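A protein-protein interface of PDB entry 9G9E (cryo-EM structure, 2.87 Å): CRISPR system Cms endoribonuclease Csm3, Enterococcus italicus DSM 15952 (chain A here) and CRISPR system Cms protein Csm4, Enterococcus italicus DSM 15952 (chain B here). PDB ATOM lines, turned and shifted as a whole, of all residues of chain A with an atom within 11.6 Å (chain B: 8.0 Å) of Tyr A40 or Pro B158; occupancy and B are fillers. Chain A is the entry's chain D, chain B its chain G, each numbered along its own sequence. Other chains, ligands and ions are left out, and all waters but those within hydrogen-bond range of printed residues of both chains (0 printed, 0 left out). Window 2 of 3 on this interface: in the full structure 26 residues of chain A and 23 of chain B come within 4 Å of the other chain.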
ATOM      1  N   VAL A  35     -21.138   4.418  -6.956  1.00  0.00           N
ATOM      2  CA  VAL A  35     -19.839   5.064  -7.061  1.00  0.00           C
ATOM      3  C   VAL A  35     -19.984   6.536  -6.693  1.00  0.00           C
ATOM      4  O   VAL A  35     -21.079   7.103  -6.698  1.00  0.00           O
ATOM      5  CB  VAL A  35     -19.234   4.902  -8.469  1.00  0.00           C
ATOM      6  CG1 VAL A  35     -18.785   3.470  -8.691  1.00  0.00           C
ATOM      7  CG2 VAL A  35     -20.236   5.323  -9.531  1.00  0.00           C
ATOM      8  N   VAL A  36     -18.858   7.161  -6.367  1.00  0.00           N
ATOM      9  CA  VAL A  36     -18.837   8.582  -6.040  1.00  0.00           C
ATOM     10  C   VAL A  36     -19.079   9.382  -7.313  1.00  0.00           C
ATOM     11  O   VAL A  36     -18.586   9.030  -8.392  1.00  0.00           O
ATOM     12  CB  VAL A  36     -17.504   8.958  -5.367  1.00  0.00           C
ATOM     13  CG1 VAL A  36     -16.329   8.526  -6.228  1.00  0.00           C
ATOM     14  CG2 VAL A  36     -17.445  10.449  -5.073  1.00  0.00           C
ATOM     15  N   ARG A  37     -19.852  10.460  -7.196  1.00  0.00           N
ATOM     16  CA  ARG A  37     -20.276  11.225  -8.358  1.00  0.00           C
ATOM     17  C   ARG A  37     -20.169  12.715  -8.070  1.00  0.00           C
ATOM     18  O   ARG A  37     -20.125  13.149  -6.917  1.00  0.00           O
ATOM     19  CB  ARG A  37     -21.717  10.888  -8.761  1.00  0.00           C
ATOM     20  CG  ARG A  37     -21.842  10.146 -10.075  1.00  0.00           C
ATOM     21  CD  ARG A  37     -23.277   9.728 -10.321  1.00  0.00           C
ATOM     22  NE  ARG A  37     -23.589   8.434  -9.731  1.00  0.00           N
ATOM     23  CZ  ARG A  37     -23.799   7.326 -10.428  1.00  0.00           C
ATOM     24  NH1 ARG A  37     -23.722   7.315 -11.748  1.00  0.00           N
ATOM     25  NH2 ARG A  37     -24.098   6.202  -9.783  1.00  0.00           N
ATOM     26  N   ASP A  38     -20.125  13.491  -9.145  1.00  0.00           N
ATOM     27  CA  ASP A  38     -20.215  14.940  -9.032  1.00  0.00           C
ATOM     28  C   ASP A  38     -21.630  15.313  -8.602  1.00  0.00           C
ATOM     29  O   ASP A  38     -22.598  14.875  -9.233  1.00  0.00           O
ATOM     30  CB  ASP A  38     -19.867  15.590 -10.372  1.00  0.00           C
ATOM     31  CG  ASP A  38     -19.795  17.106 -10.297  1.00  0.00           C
ATOM     32  OD1 ASP A  38     -19.725  17.657  -9.181  1.00  0.00           O
ATOM     33  OD2 ASP A  38     -19.802  17.752 -11.364  1.00  0.00           O
ATOM     34  N   PRO A  39     -21.797  16.089  -7.527  1.00  0.00           N
ATOM     35  CA  PRO A  39     -23.158  16.408  -7.063  1.00  0.00           C
ATOM     36  C   PRO A  39     -24.022  17.105  -8.100  1.00  0.00           C
ATOM     37  O   PRO A  39     -25.243  16.903  -8.105  1.00  0.00           O
ATOM     38  CB  PRO A  39     -22.904  17.308  -5.846  1.00  0.00           C
ATOM     39  CG  PRO A  39     -21.568  16.890  -5.351  1.00  0.00           C
ATOM     40  CD  PRO A  39     -20.768  16.510  -6.560  1.00  0.00           C
ATOM     41  N   TYR A  40     -23.437  17.916  -8.980  1.00  0.00           N
ATOM     42  CA  TYR A  40     -24.231  18.679  -9.939  1.00  0.00           C
ATOM     43  C   TYR A  40     -24.489  17.898 -11.225  1.00  0.00           C
ATOM     44  O   TYR A  40     -25.643  17.639 -11.579  1.00  0.00           O
ATOM     45  CB  TYR A  40     -23.534  20.008 -10.256  1.00  0.00           C
ATOM     46  CG  TYR A  40     -24.030  20.661 -11.526  1.00  0.00           C
ATOM     47  CD1 TYR A  40     -25.345  21.092 -11.639  1.00  0.00           C
ATOM     48  CD2 TYR A  40     -23.187  20.839 -12.613  1.00  0.00           C
ATOM     49  CE1 TYR A  40     -25.803  21.689 -12.798  1.00  0.00           C
ATOM     50  CE2 TYR A  40     -23.637  21.432 -13.775  1.00  0.00           C
ATOM     51  CZ  TYR A  40     -24.946  21.855 -13.861  1.00  0.00           C
ATOM     52  OH  TYR A  40     -25.398  22.447 -15.018  1.00  0.00           O
ATOM     53  N   SER A  41     -23.425  17.514 -11.932  1.00  0.00           N
ATOM     54  CA  SER A  41     -23.575  16.849 -13.220  1.00  0.00           C
ATOM     55  C   SER A  41     -23.895  15.367 -13.095  1.00  0.00           C
ATOM     56  O   SER A  41     -24.235  14.741 -14.106  1.00  0.00           O
ATOM     57  CB  SER A  41     -22.306  17.028 -14.057  1.00  0.00           C
ATOM     58  OG  SER A  41     -21.189  16.431 -13.425  1.00  0.00           O
ATOM     59  N   ARG A  42     -23.797  14.799 -11.892  1.00  0.00           N
ATOM     60  CA  ARG A  42     -24.053  13.378 -11.655  1.00  0.00           C
ATOM     61  C   ARG A  42     -23.169  12.502 -12.541  1.00  0.00           C
ATOM     62  O   ARG A  42     -23.604  11.477 -13.070  1.00  0.00           O
ATOM     63  CB  ARG A  42     -25.534  13.038 -11.850  1.00  0.00           C
ATOM     64  CG  ARG A  42     -26.037  11.951 -10.917  1.00  0.00           C
ATOM     65  CD  ARG A  42     -27.301  11.287 -11.447  1.00  0.00           C
ATOM     66  NE  ARG A  42     -27.480   9.926 -10.950  1.00  0.00           N
ATOM     67  CZ  ARG A  42     -27.610   9.588  -9.672  1.00  0.00           C
ATOM     68  NH1 ARG A  42     -27.641  10.497  -8.712  1.00  0.00           N
ATOM     69  NH2 ARG A  42     -27.726   8.303  -9.352  1.00  0.00           N
ATOM     70  N   LEU A  43     -21.911  12.915 -12.705  1.00  0.00           N
ATOM     71  CA  LEU A  43     -20.888  12.244 -13.487  1.00  0.00           C
ATOM     72  C   LEU A  43     -19.905  11.522 -12.575  1.00  0.00           C
ATOM     73  O   LEU A  43     -19.553  12.031 -11.508  1.00  0.00           O
ATOM     74  CB  LEU A  43     -20.125  13.251 -14.350  1.00  0.00           C
ATOM     75  CG  LEU A  43     -20.833  13.771 -15.598  1.00  0.00           C
ATOM     76  CD1 LEU A  43     -19.968  14.806 -16.287  1.00  0.00           C
ATOM     77  CD2 LEU A  43     -21.154  12.628 -16.540  1.00  0.00           C
ATOM     78  N   PRO A  44     -19.445  10.333 -12.965  1.00  0.00           N
ATOM     79  CA  PRO A  44     -18.455   9.628 -12.143  1.00  0.00           C
ATOM     80  C   PRO A  44     -17.179  10.442 -12.000  1.00  0.00           C
ATOM     81  O   PRO A  44     -16.736  11.114 -12.933  1.00  0.00           O
ATOM     82  CB  PRO A  44     -18.207   8.329 -12.919  1.00  0.00           C
ATOM     83  CG  PRO A  44     -19.430   8.150 -13.757  1.00  0.00           C
ATOM     84  CD  PRO A  44     -19.873   9.533 -14.124  1.00  0.00           C
ATOM     85  N   ILE A  45     -16.594  10.386 -10.804  1.00  0.00           N
ATOM     86  CA  ILE A  45     -15.362  11.098 -10.502  1.00  0.00           C
ATOM     87  C   ILE A  45     -14.412  10.164  -9.768  1.00  0.00           C
ATOM     88  O   ILE A  45     -14.815   9.161  -9.176  1.00  0.00           O
ATOM     89  CB  ILE A  45     -15.601  12.373  -9.661  1.00  0.00           C
ATOM     90  CG1 ILE A  45     -16.124  12.008  -8.270  1.00  0.00           C
ATOM     91  CG2 ILE A  45     -16.552  13.325 -10.371  1.00  0.00           C
ATOM     92  CD1 ILE A  45     -16.254  13.189  -7.339  1.00  0.00           C
ATOM     93  N   ASP A 100      -9.509  16.296  -8.005  1.00  0.00           N
ATOM     94  CA  ASP A 100     -10.435  15.252  -8.417  1.00  0.00           C
ATOM     95  C   ASP A 100     -10.387  15.066  -9.927  1.00  0.00           C
ATOM     96  O   ASP A 100     -10.331  16.036 -10.689  1.00  0.00           O
ATOM     97  CB  ASP A 100     -11.859  15.597  -7.976  1.00  0.00           C
ATOM     98  CG  ASP A 100     -12.054  15.478  -6.476  1.00  0.00           C
ATOM     99  OD1 ASP A 100     -11.086  15.708  -5.722  1.00  0.00           O
ATOM    100  OD2 ASP A 100     -13.182  15.155  -6.049  1.00  0.00           O
ATOM    101  N   PHE A 102     -12.254  14.299 -13.142  1.00  0.00           N
ATOM    102  CA  PHE A 102     -13.622  14.393 -13.624  1.00  0.00           C
ATOM    103  C   PHE A 102     -13.771  13.638 -14.937  1.00  0.00           C
ATOM    104  O   PHE A 102     -12.813  13.484 -15.697  1.00  0.00           O
ATOM    105  CB  PHE A 102     -14.032  15.854 -13.812  1.00  0.00           C
ATOM    106  CG  PHE A 102     -13.815  16.700 -12.592  1.00  0.00           C
ATOM    107  CD1 PHE A 102     -14.697  16.642 -11.527  1.00  0.00           C
ATOM    108  CD2 PHE A 102     -12.724  17.546 -12.506  1.00  0.00           C
ATOM    109  CE1 PHE A 102     -14.497  17.415 -10.402  1.00  0.00           C
ATOM    110  CE2 PHE A 102     -12.518  18.323 -11.383  1.00  0.00           C
ATOM    111  CZ  PHE A 102     -13.406  18.256 -10.330  1.00  0.00           C
ATOM    112  N   PHE A 103     -14.984  13.151 -15.184  1.00  0.00           N
ATOM    113  CA  PHE A 103     -15.280  12.422 -16.411  1.00  0.00           C
ATOM    114  C   PHE A 103     -14.930  13.270 -17.625  1.00  0.00           C
ATOM    115  O   PHE A 103     -15.402  14.403 -17.761  1.00  0.00           O
ATOM    116  CB  PHE A 103     -16.760  12.033 -16.434  1.00  0.00           C
ATOM    117  CG  PHE A 103     -17.045  10.774 -17.197  1.00  0.00           C
ATOM    118  CD1 PHE A 103     -16.893   9.538 -16.595  1.00  0.00           C
ATOM    119  CD2 PHE A 103     -17.474  10.824 -18.512  1.00  0.00           C
ATOM    120  CE1 PHE A 103     -17.157   8.375 -17.289  1.00  0.00           C
ATOM    121  CE2 PHE A 103     -17.740   9.663 -19.213  1.00  0.00           C
ATOM    122  CZ  PHE A 103     -17.581   8.437 -18.600  1.00  0.00           C
ATOM    123  N   LYS A 105     -14.546  14.972 -21.282  1.00  0.00           N
ATOM    124  CA  LYS A 105     -15.562  15.411 -22.232  1.00  0.00           C
ATOM    125  C   LYS A 105     -15.527  14.575 -23.505  1.00  0.00           C
ATOM    126  O   LYS A 105     -16.577  14.259 -24.077  1.00  0.00           O
ATOM    127  CB  LYS A 105     -15.376  16.893 -22.555  1.00  0.00           C
ATOM    128  CG  LYS A 105     -16.439  17.463 -23.481  1.00  0.00           C
ATOM    129  CD  LYS A 105     -17.834  17.201 -22.933  1.00  0.00           C
ATOM    130  CE  LYS A 105     -18.907  17.524 -23.960  1.00  0.00           C
ATOM    131  NZ  LYS A 105     -20.267  17.167 -23.468  1.00  0.00           N
ATOM    132  N   GLN A 108     -17.095  11.548 -22.613  1.00  0.00           N
ATOM    133  CA  GLN A 108     -18.523  11.829 -22.509  1.00  0.00           C
ATOM    134  C   GLN A 108     -19.203  11.737 -23.868  1.00  0.00           C
ATOM    135  O   GLN A 108     -20.262  11.115 -23.999  1.00  0.00           O
ATOM    136  CB  GLN A 108     -18.736  13.216 -21.905  1.00  0.00           C
ATOM    137  CG  GLN A 108     -19.391  13.222 -20.540  1.00  0.00           C
ATOM    138  CD  GLN A 108     -19.764  14.620 -20.097  1.00  0.00           C
ATOM    139  OE1 GLN A 108     -19.072  15.231 -19.285  1.00  0.00           O
ATOM    140  NE2 GLN A 108     -20.865  15.136 -20.630  1.00  0.00           N
ATOM    141  N   TYR A 118     -22.575   5.607 -18.514  1.00  0.00           N
ATOM    142  CA  TYR A 118     -21.271   5.873 -17.918  1.00  0.00           C
ATOM    143  C   TYR A 118     -20.908   4.833 -16.868  1.00  0.00           C
ATOM    144  O   TYR A 118     -19.722   4.554 -16.658  1.00  0.00           O
ATOM    145  CB  TYR A 118     -21.247   7.272 -17.305  1.00  0.00           C
ATOM    146  CG  TYR A 118     -21.639   8.370 -18.266  1.00  0.00           C
ATOM    147  CD1 TYR A 118     -21.180   8.369 -19.575  1.00  0.00           C
ATOM    148  CD2 TYR A 118     -22.466   9.409 -17.862  1.00  0.00           C
ATOM    149  CE1 TYR A 118     -21.537   9.371 -20.457  1.00  0.00           C
ATOM    150  CE2 TYR A 118     -22.827  10.415 -18.736  1.00  0.00           C
ATOM    151  CZ  TYR A 118     -22.360  10.391 -20.031  1.00  0.00           C
ATOM    152  OH  TYR A 118     -22.716  11.390 -20.905  1.00  0.00           O
ATOM    153  N   THR B  12     -13.708  31.303 -10.926  1.00  0.00           N
ATOM    154  CA  THR B  12     -14.463  30.148 -11.390  1.00  0.00           C
ATOM    155  C   THR B  12     -13.743  28.893 -10.919  1.00  0.00           C
ATOM    156  O   THR B  12     -12.533  28.749 -11.126  1.00  0.00           O
ATOM    157  CB  THR B  12     -14.606  30.150 -12.914  1.00  0.00           C
ATOM    158  OG1 THR B  12     -13.461  29.533 -13.514  1.00  0.00           O
ATOM    159  CG2 THR B  12     -14.726  31.573 -13.435  1.00  0.00           C
ATOM    160  N   PHE B  13     -14.481  27.991 -10.284  1.00  0.00           N
ATOM    161  CA  PHE B  13     -13.888  26.880  -9.556  1.00  0.00           C
ATOM    162  C   PHE B  13     -14.006  25.603 -10.374  1.00  0.00           C
ATOM    163  O   PHE B  13     -15.095  25.259 -10.845  1.00  0.00           O
ATOM    164  CB  PHE B  13     -14.561  26.717  -8.192  1.00  0.00           C
ATOM    165  CG  PHE B  13     -14.292  27.858  -7.253  1.00  0.00           C
ATOM    166  CD1 PHE B  13     -15.106  28.978  -7.257  1.00  0.00           C
ATOM    167  CD2 PHE B  13     -13.214  27.825  -6.391  1.00  0.00           C
ATOM    168  CE1 PHE B  13     -14.859  30.033  -6.403  1.00  0.00           C
ATOM    169  CE2 PHE B  13     -12.962  28.876  -5.534  1.00  0.00           C
ATOM    170  CZ  PHE B  13     -13.785  29.982  -5.541  1.00  0.00           C
ATOM    171  N   LYS B  14     -12.881  24.907 -10.538  1.00  0.00           N
ATOM    172  CA  LYS B  14     -12.868  23.659 -11.294  1.00  0.00           C
ATOM    173  C   LYS B  14     -13.423  22.513 -10.457  1.00  0.00           C
ATOM    174  O   LYS B  14     -14.407  21.869 -10.834  1.00  0.00           O
ATOM    175  CB  LYS B  14     -11.443  23.343 -11.756  1.00  0.00           C
ATOM    176  CG  LYS B  14     -10.578  24.566 -12.035  1.00  0.00           C
ATOM    177  CD  LYS B  14     -10.826  25.141 -13.421  1.00  0.00           C
ATOM    178  CE  LYS B  14     -11.734  26.359 -13.371  1.00  0.00           C
ATOM    179  NZ  LYS B  14     -11.965  26.935 -14.723  1.00  0.00           N
ATOM    180  N   TYR B  66     -21.830  34.882  -7.633  1.00  0.00           N
ATOM    181  CA  TYR B  66     -22.268  35.419  -8.912  1.00  0.00           C
ATOM    182  C   TYR B  66     -22.687  34.263  -9.808  1.00  0.00           C
ATOM    183  O   TYR B  66     -22.103  33.176  -9.764  1.00  0.00           O
ATOM    184  CB  TYR B  66     -21.184  36.280  -9.588  1.00  0.00           C
ATOM    185  CG  TYR B  66     -20.069  35.527 -10.288  1.00  0.00           C
ATOM    186  CD1 TYR B  66     -20.241  35.013 -11.568  1.00  0.00           C
ATOM    187  CD2 TYR B  66     -18.834  35.361  -9.682  1.00  0.00           C
ATOM    188  CE1 TYR B  66     -19.227  34.333 -12.207  1.00  0.00           C
ATOM    189  CE2 TYR B  66     -17.811  34.686 -10.318  1.00  0.00           C
ATOM    190  CZ  TYR B  66     -18.014  34.173 -11.578  1.00  0.00           C
ATOM    191  OH  TYR B  66     -16.999  33.500 -12.215  1.00  0.00           O
ATOM    192  N   ASN B  67     -23.709  34.517 -10.623  1.00  0.00           N
ATOM    193  CA  ASN B  67     -24.231  33.525 -11.553  1.00  0.00           C
ATOM    194  C   ASN B  67     -24.275  34.083 -12.971  1.00  0.00           C
ATOM    195  O   ASN B  67     -23.687  35.133 -13.246  1.00  0.00           O
ATOM    196  CB  ASN B  67     -25.615  33.041 -11.106  1.00  0.00           C
ATOM    197  CG  ASN B  67     -26.619  34.170 -10.948  1.00  0.00           C
ATOM    198  OD1 ASN B  67     -26.437  35.267 -11.474  1.00  0.00           O
ATOM    199  ND2 ASN B  67     -27.693  33.900 -10.216  1.00  0.00           N
ATOM    200  N   LYS B  68     -24.958  33.375 -13.874  1.00  0.00           N
ATOM    201  CA  LYS B  68     -24.977  33.768 -15.280  1.00  0.00           C
ATOM    202  C   LYS B  68     -25.515  35.180 -15.472  1.00  0.00           C
ATOM    203  O   LYS B  68     -25.078  35.890 -16.385  1.00  0.00           O
ATOM    204  CB  LYS B  68     -25.816  32.798 -16.131  1.00  0.00           C
ATOM    205  CG  LYS B  68     -25.693  31.273 -15.905  1.00  0.00           C
ATOM    206  CD  LYS B  68     -26.118  30.761 -14.529  1.00  0.00           C
ATOM    207  CE  LYS B  68     -25.536  29.384 -14.252  1.00  0.00           C
ATOM    208  NZ  LYS B  68     -25.795  28.940 -12.856  1.00  0.00           N
ATOM    209  N   ASN B 125     -28.257  30.997  -7.942  1.00  0.00           N
ATOM    210  CA  ASN B 125     -27.953  29.709  -8.549  1.00  0.00           C
ATOM    211  C   ASN B 125     -26.478  29.384  -8.371  1.00  0.00           C
ATOM    212  O   ASN B 125     -25.789  29.055  -9.340  1.00  0.00           O
ATOM    213  CB  ASN B 125     -28.330  29.711 -10.032  1.00  0.00           C
ATOM    214  CG  ASN B 125     -29.828  29.792 -10.254  1.00  0.00           C
ATOM    215  OD1 ASN B 125     -30.318  30.688 -10.943  1.00  0.00           O
ATOM    216  ND2 ASN B 125     -30.564  28.855  -9.668  1.00  0.00           N
ATOM    217  N   LEU B 126     -25.982  29.497  -7.138  1.00  0.00           N
ATOM    218  CA  LEU B 126     -24.557  29.308  -6.888  1.00  0.00           C
ATOM    219  C   LEU B 126     -24.126  27.875  -7.184  1.00  0.00           C
ATOM    220  O   LEU B 126     -23.272  27.639  -8.047  1.00  0.00           O
ATOM    221  CB  LEU B 126     -24.223  29.690  -5.447  1.00  0.00           C
ATOM    222  CG  LEU B 126     -22.766  30.089  -5.216  1.00  0.00           C
ATOM    223  CD1 LEU B 126     -22.302  31.054  -6.292  1.00  0.00           C
ATOM    224  CD2 LEU B 126     -22.595  30.699  -3.841  1.00  0.00           C
ATOM    225  N   GLY B 127     -24.700  26.906  -6.486  1.00  0.00           N
ATOM    226  CA  GLY B 127     -24.310  25.530  -6.704  1.00  0.00           C
ATOM    227  C   GLY B 127     -24.940  24.601  -5.688  1.00  0.00           C
ATOM    228  O   GLY B 127     -25.921  24.940  -5.022  1.00  0.00           O
ATOM    229  N   LYS B 128     -24.345  23.414  -5.591  1.00  0.00           N
ATOM    230  CA  LYS B 128     -24.844  22.328  -4.759  1.00  0.00           C
ATOM    231  C   LYS B 128     -23.832  22.007  -3.669  1.00  0.00           C
ATOM    232  O   LYS B 128     -22.643  21.830  -3.952  1.00  0.00           O
ATOM    233  CB  LYS B 128     -25.124  21.081  -5.603  1.00  0.00           C
ATOM    234  CG  LYS B 128     -25.873  19.982  -4.871  1.00  0.00           C
ATOM    235  CD  LYS B 128     -27.375  20.189  -4.950  1.00  0.00           C
ATOM    236  CE  LYS B 128     -28.055  19.787  -3.652  1.00  0.00           C
ATOM    237  NZ  LYS B 128     -28.429  20.971  -2.831  1.00  0.00           N
ATOM    238  N   ALA B 129     -24.308  21.928  -2.430  1.00  0.00           N
ATOM    239  CA  ALA B 129     -23.487  21.534  -1.294  1.00  0.00           C
ATOM    240  C   ALA B 129     -23.714  20.057  -0.999  1.00  0.00           C
ATOM    241  O   ALA B 129     -24.860  19.610  -0.891  1.00  0.00           O
ATOM    242  CB  ALA B 129     -23.815  22.379  -0.062  1.00  0.00           C
ATOM    243  N   SER B 130     -22.623  19.306  -0.869  1.00  0.00           N
ATOM    244  CA  SER B 130     -22.686  17.872  -0.634  1.00  0.00           C
ATOM    245  C   SER B 130     -21.671  17.508   0.444  1.00  0.00           C
ATOM    246  O   SER B 130     -20.877  18.343   0.886  1.00  0.00           O
ATOM    247  CB  SER B 130     -22.439  17.094  -1.932  1.00  0.00           C
ATOM    248  OG  SER B 130     -22.474  15.692  -1.727  1.00  0.00           O
ATOM    249  N   THR B 155     -19.960  22.494  -4.859  1.00  0.00           N
ATOM    250  CA  THR B 155     -19.619  22.589  -6.271  1.00  0.00           C
ATOM    251  C   THR B 155     -20.480  23.661  -6.926  1.00  0.00           C
ATOM    252  O   THR B 155     -21.688  23.743  -6.674  1.00  0.00           O
ATOM    253  CB  THR B 155     -19.771  21.230  -6.974  1.00  0.00           C
ATOM    254  OG1 THR B 155     -19.024  21.232  -8.197  1.00  0.00           O
ATOM    255  CG2 THR B 155     -21.228  20.882  -7.260  1.00  0.00           C
ATOM    256  N   PHE B 156     -19.844  24.520  -7.714  1.00  0.00           N
ATOM    257  CA  PHE B 156     -20.553  25.616  -8.352  1.00  0.00           C
ATOM    258  C   PHE B 156     -21.123  25.182  -9.699  1.00  0.00           C
ATOM    259  O   PHE B 156     -20.622  24.264 -10.354  1.00  0.00           O
ATOM    260  CB  PHE B 156     -19.633  26.825  -8.538  1.00  0.00           C
ATOM    261  CG  PHE B 156     -19.093  27.383  -7.251  1.00  0.00           C
ATOM    262  CD1 PHE B 156     -18.016  26.790  -6.615  1.00  0.00           C
ATOM    263  CD2 PHE B 156     -19.665  28.506  -6.677  1.00  0.00           C
ATOM    264  CE1 PHE B 156     -17.521  27.304  -5.433  1.00  0.00           C
ATOM    265  CE2 PHE B 156     -19.175  29.024  -5.496  1.00  0.00           C
ATOM    266  CZ  PHE B 156     -18.101  28.422  -4.874  1.00  0.00           C
ATOM    267  N   TYR B 157     -22.189  25.862 -10.106  1.00  0.00           N
ATOM    268  CA  TYR B 157     -22.785  25.630 -11.407  1.00  0.00           C
ATOM    269  C   TYR B 157     -21.854  26.169 -12.494  1.00  0.00           C
ATOM    270  O   TYR B 157     -20.965  26.976 -12.211  1.00  0.00           O
ATOM    271  CB  TYR B 157     -24.165  26.282 -11.465  1.00  0.00           C
ATOM    272  CG  TYR B 157     -25.194  25.571 -10.610  1.00  0.00           C
ATOM    273  CD1 TYR B 157     -24.989  24.265 -10.186  1.00  0.00           C
ATOM    274  CD2 TYR B 157     -26.368  26.203 -10.228  1.00  0.00           C
ATOM    275  CE1 TYR B 157     -25.921  23.611  -9.404  1.00  0.00           C
ATOM    276  CE2 TYR B 157     -27.306  25.557  -9.445  1.00  0.00           C
ATOM    277  CZ  TYR B 157     -27.078  24.262  -9.037  1.00  0.00           C
ATOM    278  OH  TYR B 157     -28.009  23.613  -8.259  1.00  0.00           O
ATOM    279  N   PRO B 158     -22.022  25.721 -13.748  1.00  0.00           N
ATOM    280  CA  PRO B 158     -20.992  26.000 -14.769  1.00  0.00           C
ATOM    281  C   PRO B 158     -20.644  27.469 -14.951  1.00  0.00           C
ATOM    282  O   PRO B 158     -19.471  27.787 -15.179  1.00  0.00           O
ATOM    283  CB  PRO B 158     -21.611  25.406 -16.041  1.00  0.00           C
ATOM    284  CG  PRO B 158     -22.478  24.314 -15.548  1.00  0.00           C
ATOM    285  CD  PRO B 158     -23.074  24.832 -14.274  1.00  0.00           C
ATOM    286  N   GLU B 159     -21.616  28.376 -14.859  1.00  0.00           N
ATOM    287  CA  GLU B 159     -21.352  29.799 -15.033  1.00  0.00           C
ATOM    288  C   GLU B 159     -21.476  30.579 -13.728  1.00  0.00           C
ATOM    289  O   GLU B 159     -21.649  31.801 -13.752  1.00  0.00           O
ATOM    290  CB  GLU B 159     -22.278  30.389 -16.095  1.00  0.00           C
ATOM    291  CG  GLU B 159     -22.049  29.833 -17.490  1.00  0.00           C
ATOM    292  CD  GLU B 159     -22.734  30.655 -18.563  1.00  0.00           C
ATOM    293  OE1 GLU B 159     -22.551  31.891 -18.574  1.00  0.00           O
ATOM    294  OE2 GLU B 159     -23.456  30.066 -19.394  1.00  0.00           O
ATOM    295  N   SER B 160     -21.392  29.897 -12.592  1.00  0.00           N
ATOM    296  CA  SER B 160     -21.396  30.540 -11.288  1.00  0.00           C
ATOM    297  C   SER B 160     -19.981  30.582 -10.720  1.00  0.00           C
ATOM    298  O   SER B 160     -19.059  29.941 -11.227  1.00  0.00           O
ATOM    299  CB  SER B 160     -22.338  29.807 -10.330  1.00  0.00           C
ATOM    300  OG  SER B 160     -23.603  29.600 -10.930  1.00  0.00           O
ATOM    301  N   GLY B 161     -19.819  31.350  -9.650  1.00  0.00           N
ATOM    302  CA  GLY B 161     -18.519  31.472  -9.027  1.00  0.00           C
ATOM    303  C   GLY B 161     -18.544  32.522  -7.936  1.00  0.00           C
ATOM    304  O   GLY B 161     -19.607  32.990  -7.523  1.00  0.00           O
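OD2 of Asp A38 lies within hydrogen-bond range of OG of Ser A41. OG1 of Thr B12 lies within hydrogen-bond range of NZ of Lys B14, 3.2 Å away. N of Tyr B157 is in hydrogen-bond range of O of Leu B126 (2.9 Å). The backbone NH (N) of Lys B128 sits at hydrogen-bond distance from the backbone carbonyl oxygen (O) of Thr B155 (2.9 Å). N of Asp A38 lies within hydrogen-bond range of O of Leu A43 (2.8 Å).
Asp A38 touches Thr B155. Pro A39 touches Ser B130 (CG to CB, 3.5 Å). CG2 of Thr B155 touches CB of Tyr A40, 3.9 Å away. CD1 of Tyr A40 touches CE1 of Tyr B157, 3.4 Å away. Tyr A40 touches Pro B158 (OH to CD, 3.4 Å). Lys B14 touches Phe A102 (O to CZ, 3.8 Å).
Of the printed residues of chain B, Asp A38 touches Thr B155 (3.8 Å). Of the printed residues of chain B, Pro A39 touches Ser B130. Of the printed residues of chain B, Phe A102 touches Lys B14 (3.8 Å). Of the printed residues of chain A, Lys B14 touches Phe A102 (3.8 Å). Of the printed residues of chain A, Ser B130 touches Pro A39 (3.5 Å). Printed residues of chain A within 4 Å of Thr B155: Asp A38 (3.8 Å) and Tyr A40 (3.9 Å). Of chain A, only Tyr A40 (3.4 Å) comes within 4 Å of Tyr B157. Pro B158 touches just one residue of chain A: Tyr A40. No residue of chain A comes within 4 Å of Ser B160. The nearest residue of chain B that does not touch Tyr A40 is Phe B156 (4.8 Å).
Hydrophobic or aromatic side chains of chain A within 4 Å of the printed part of chain B: Pro A39, Tyr A40 and Phe A102. Among the printed residues, no Asp or Glu carboxylate lies within 4 Å of a Lys or Arg side-chain nitrogen of the other chain.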
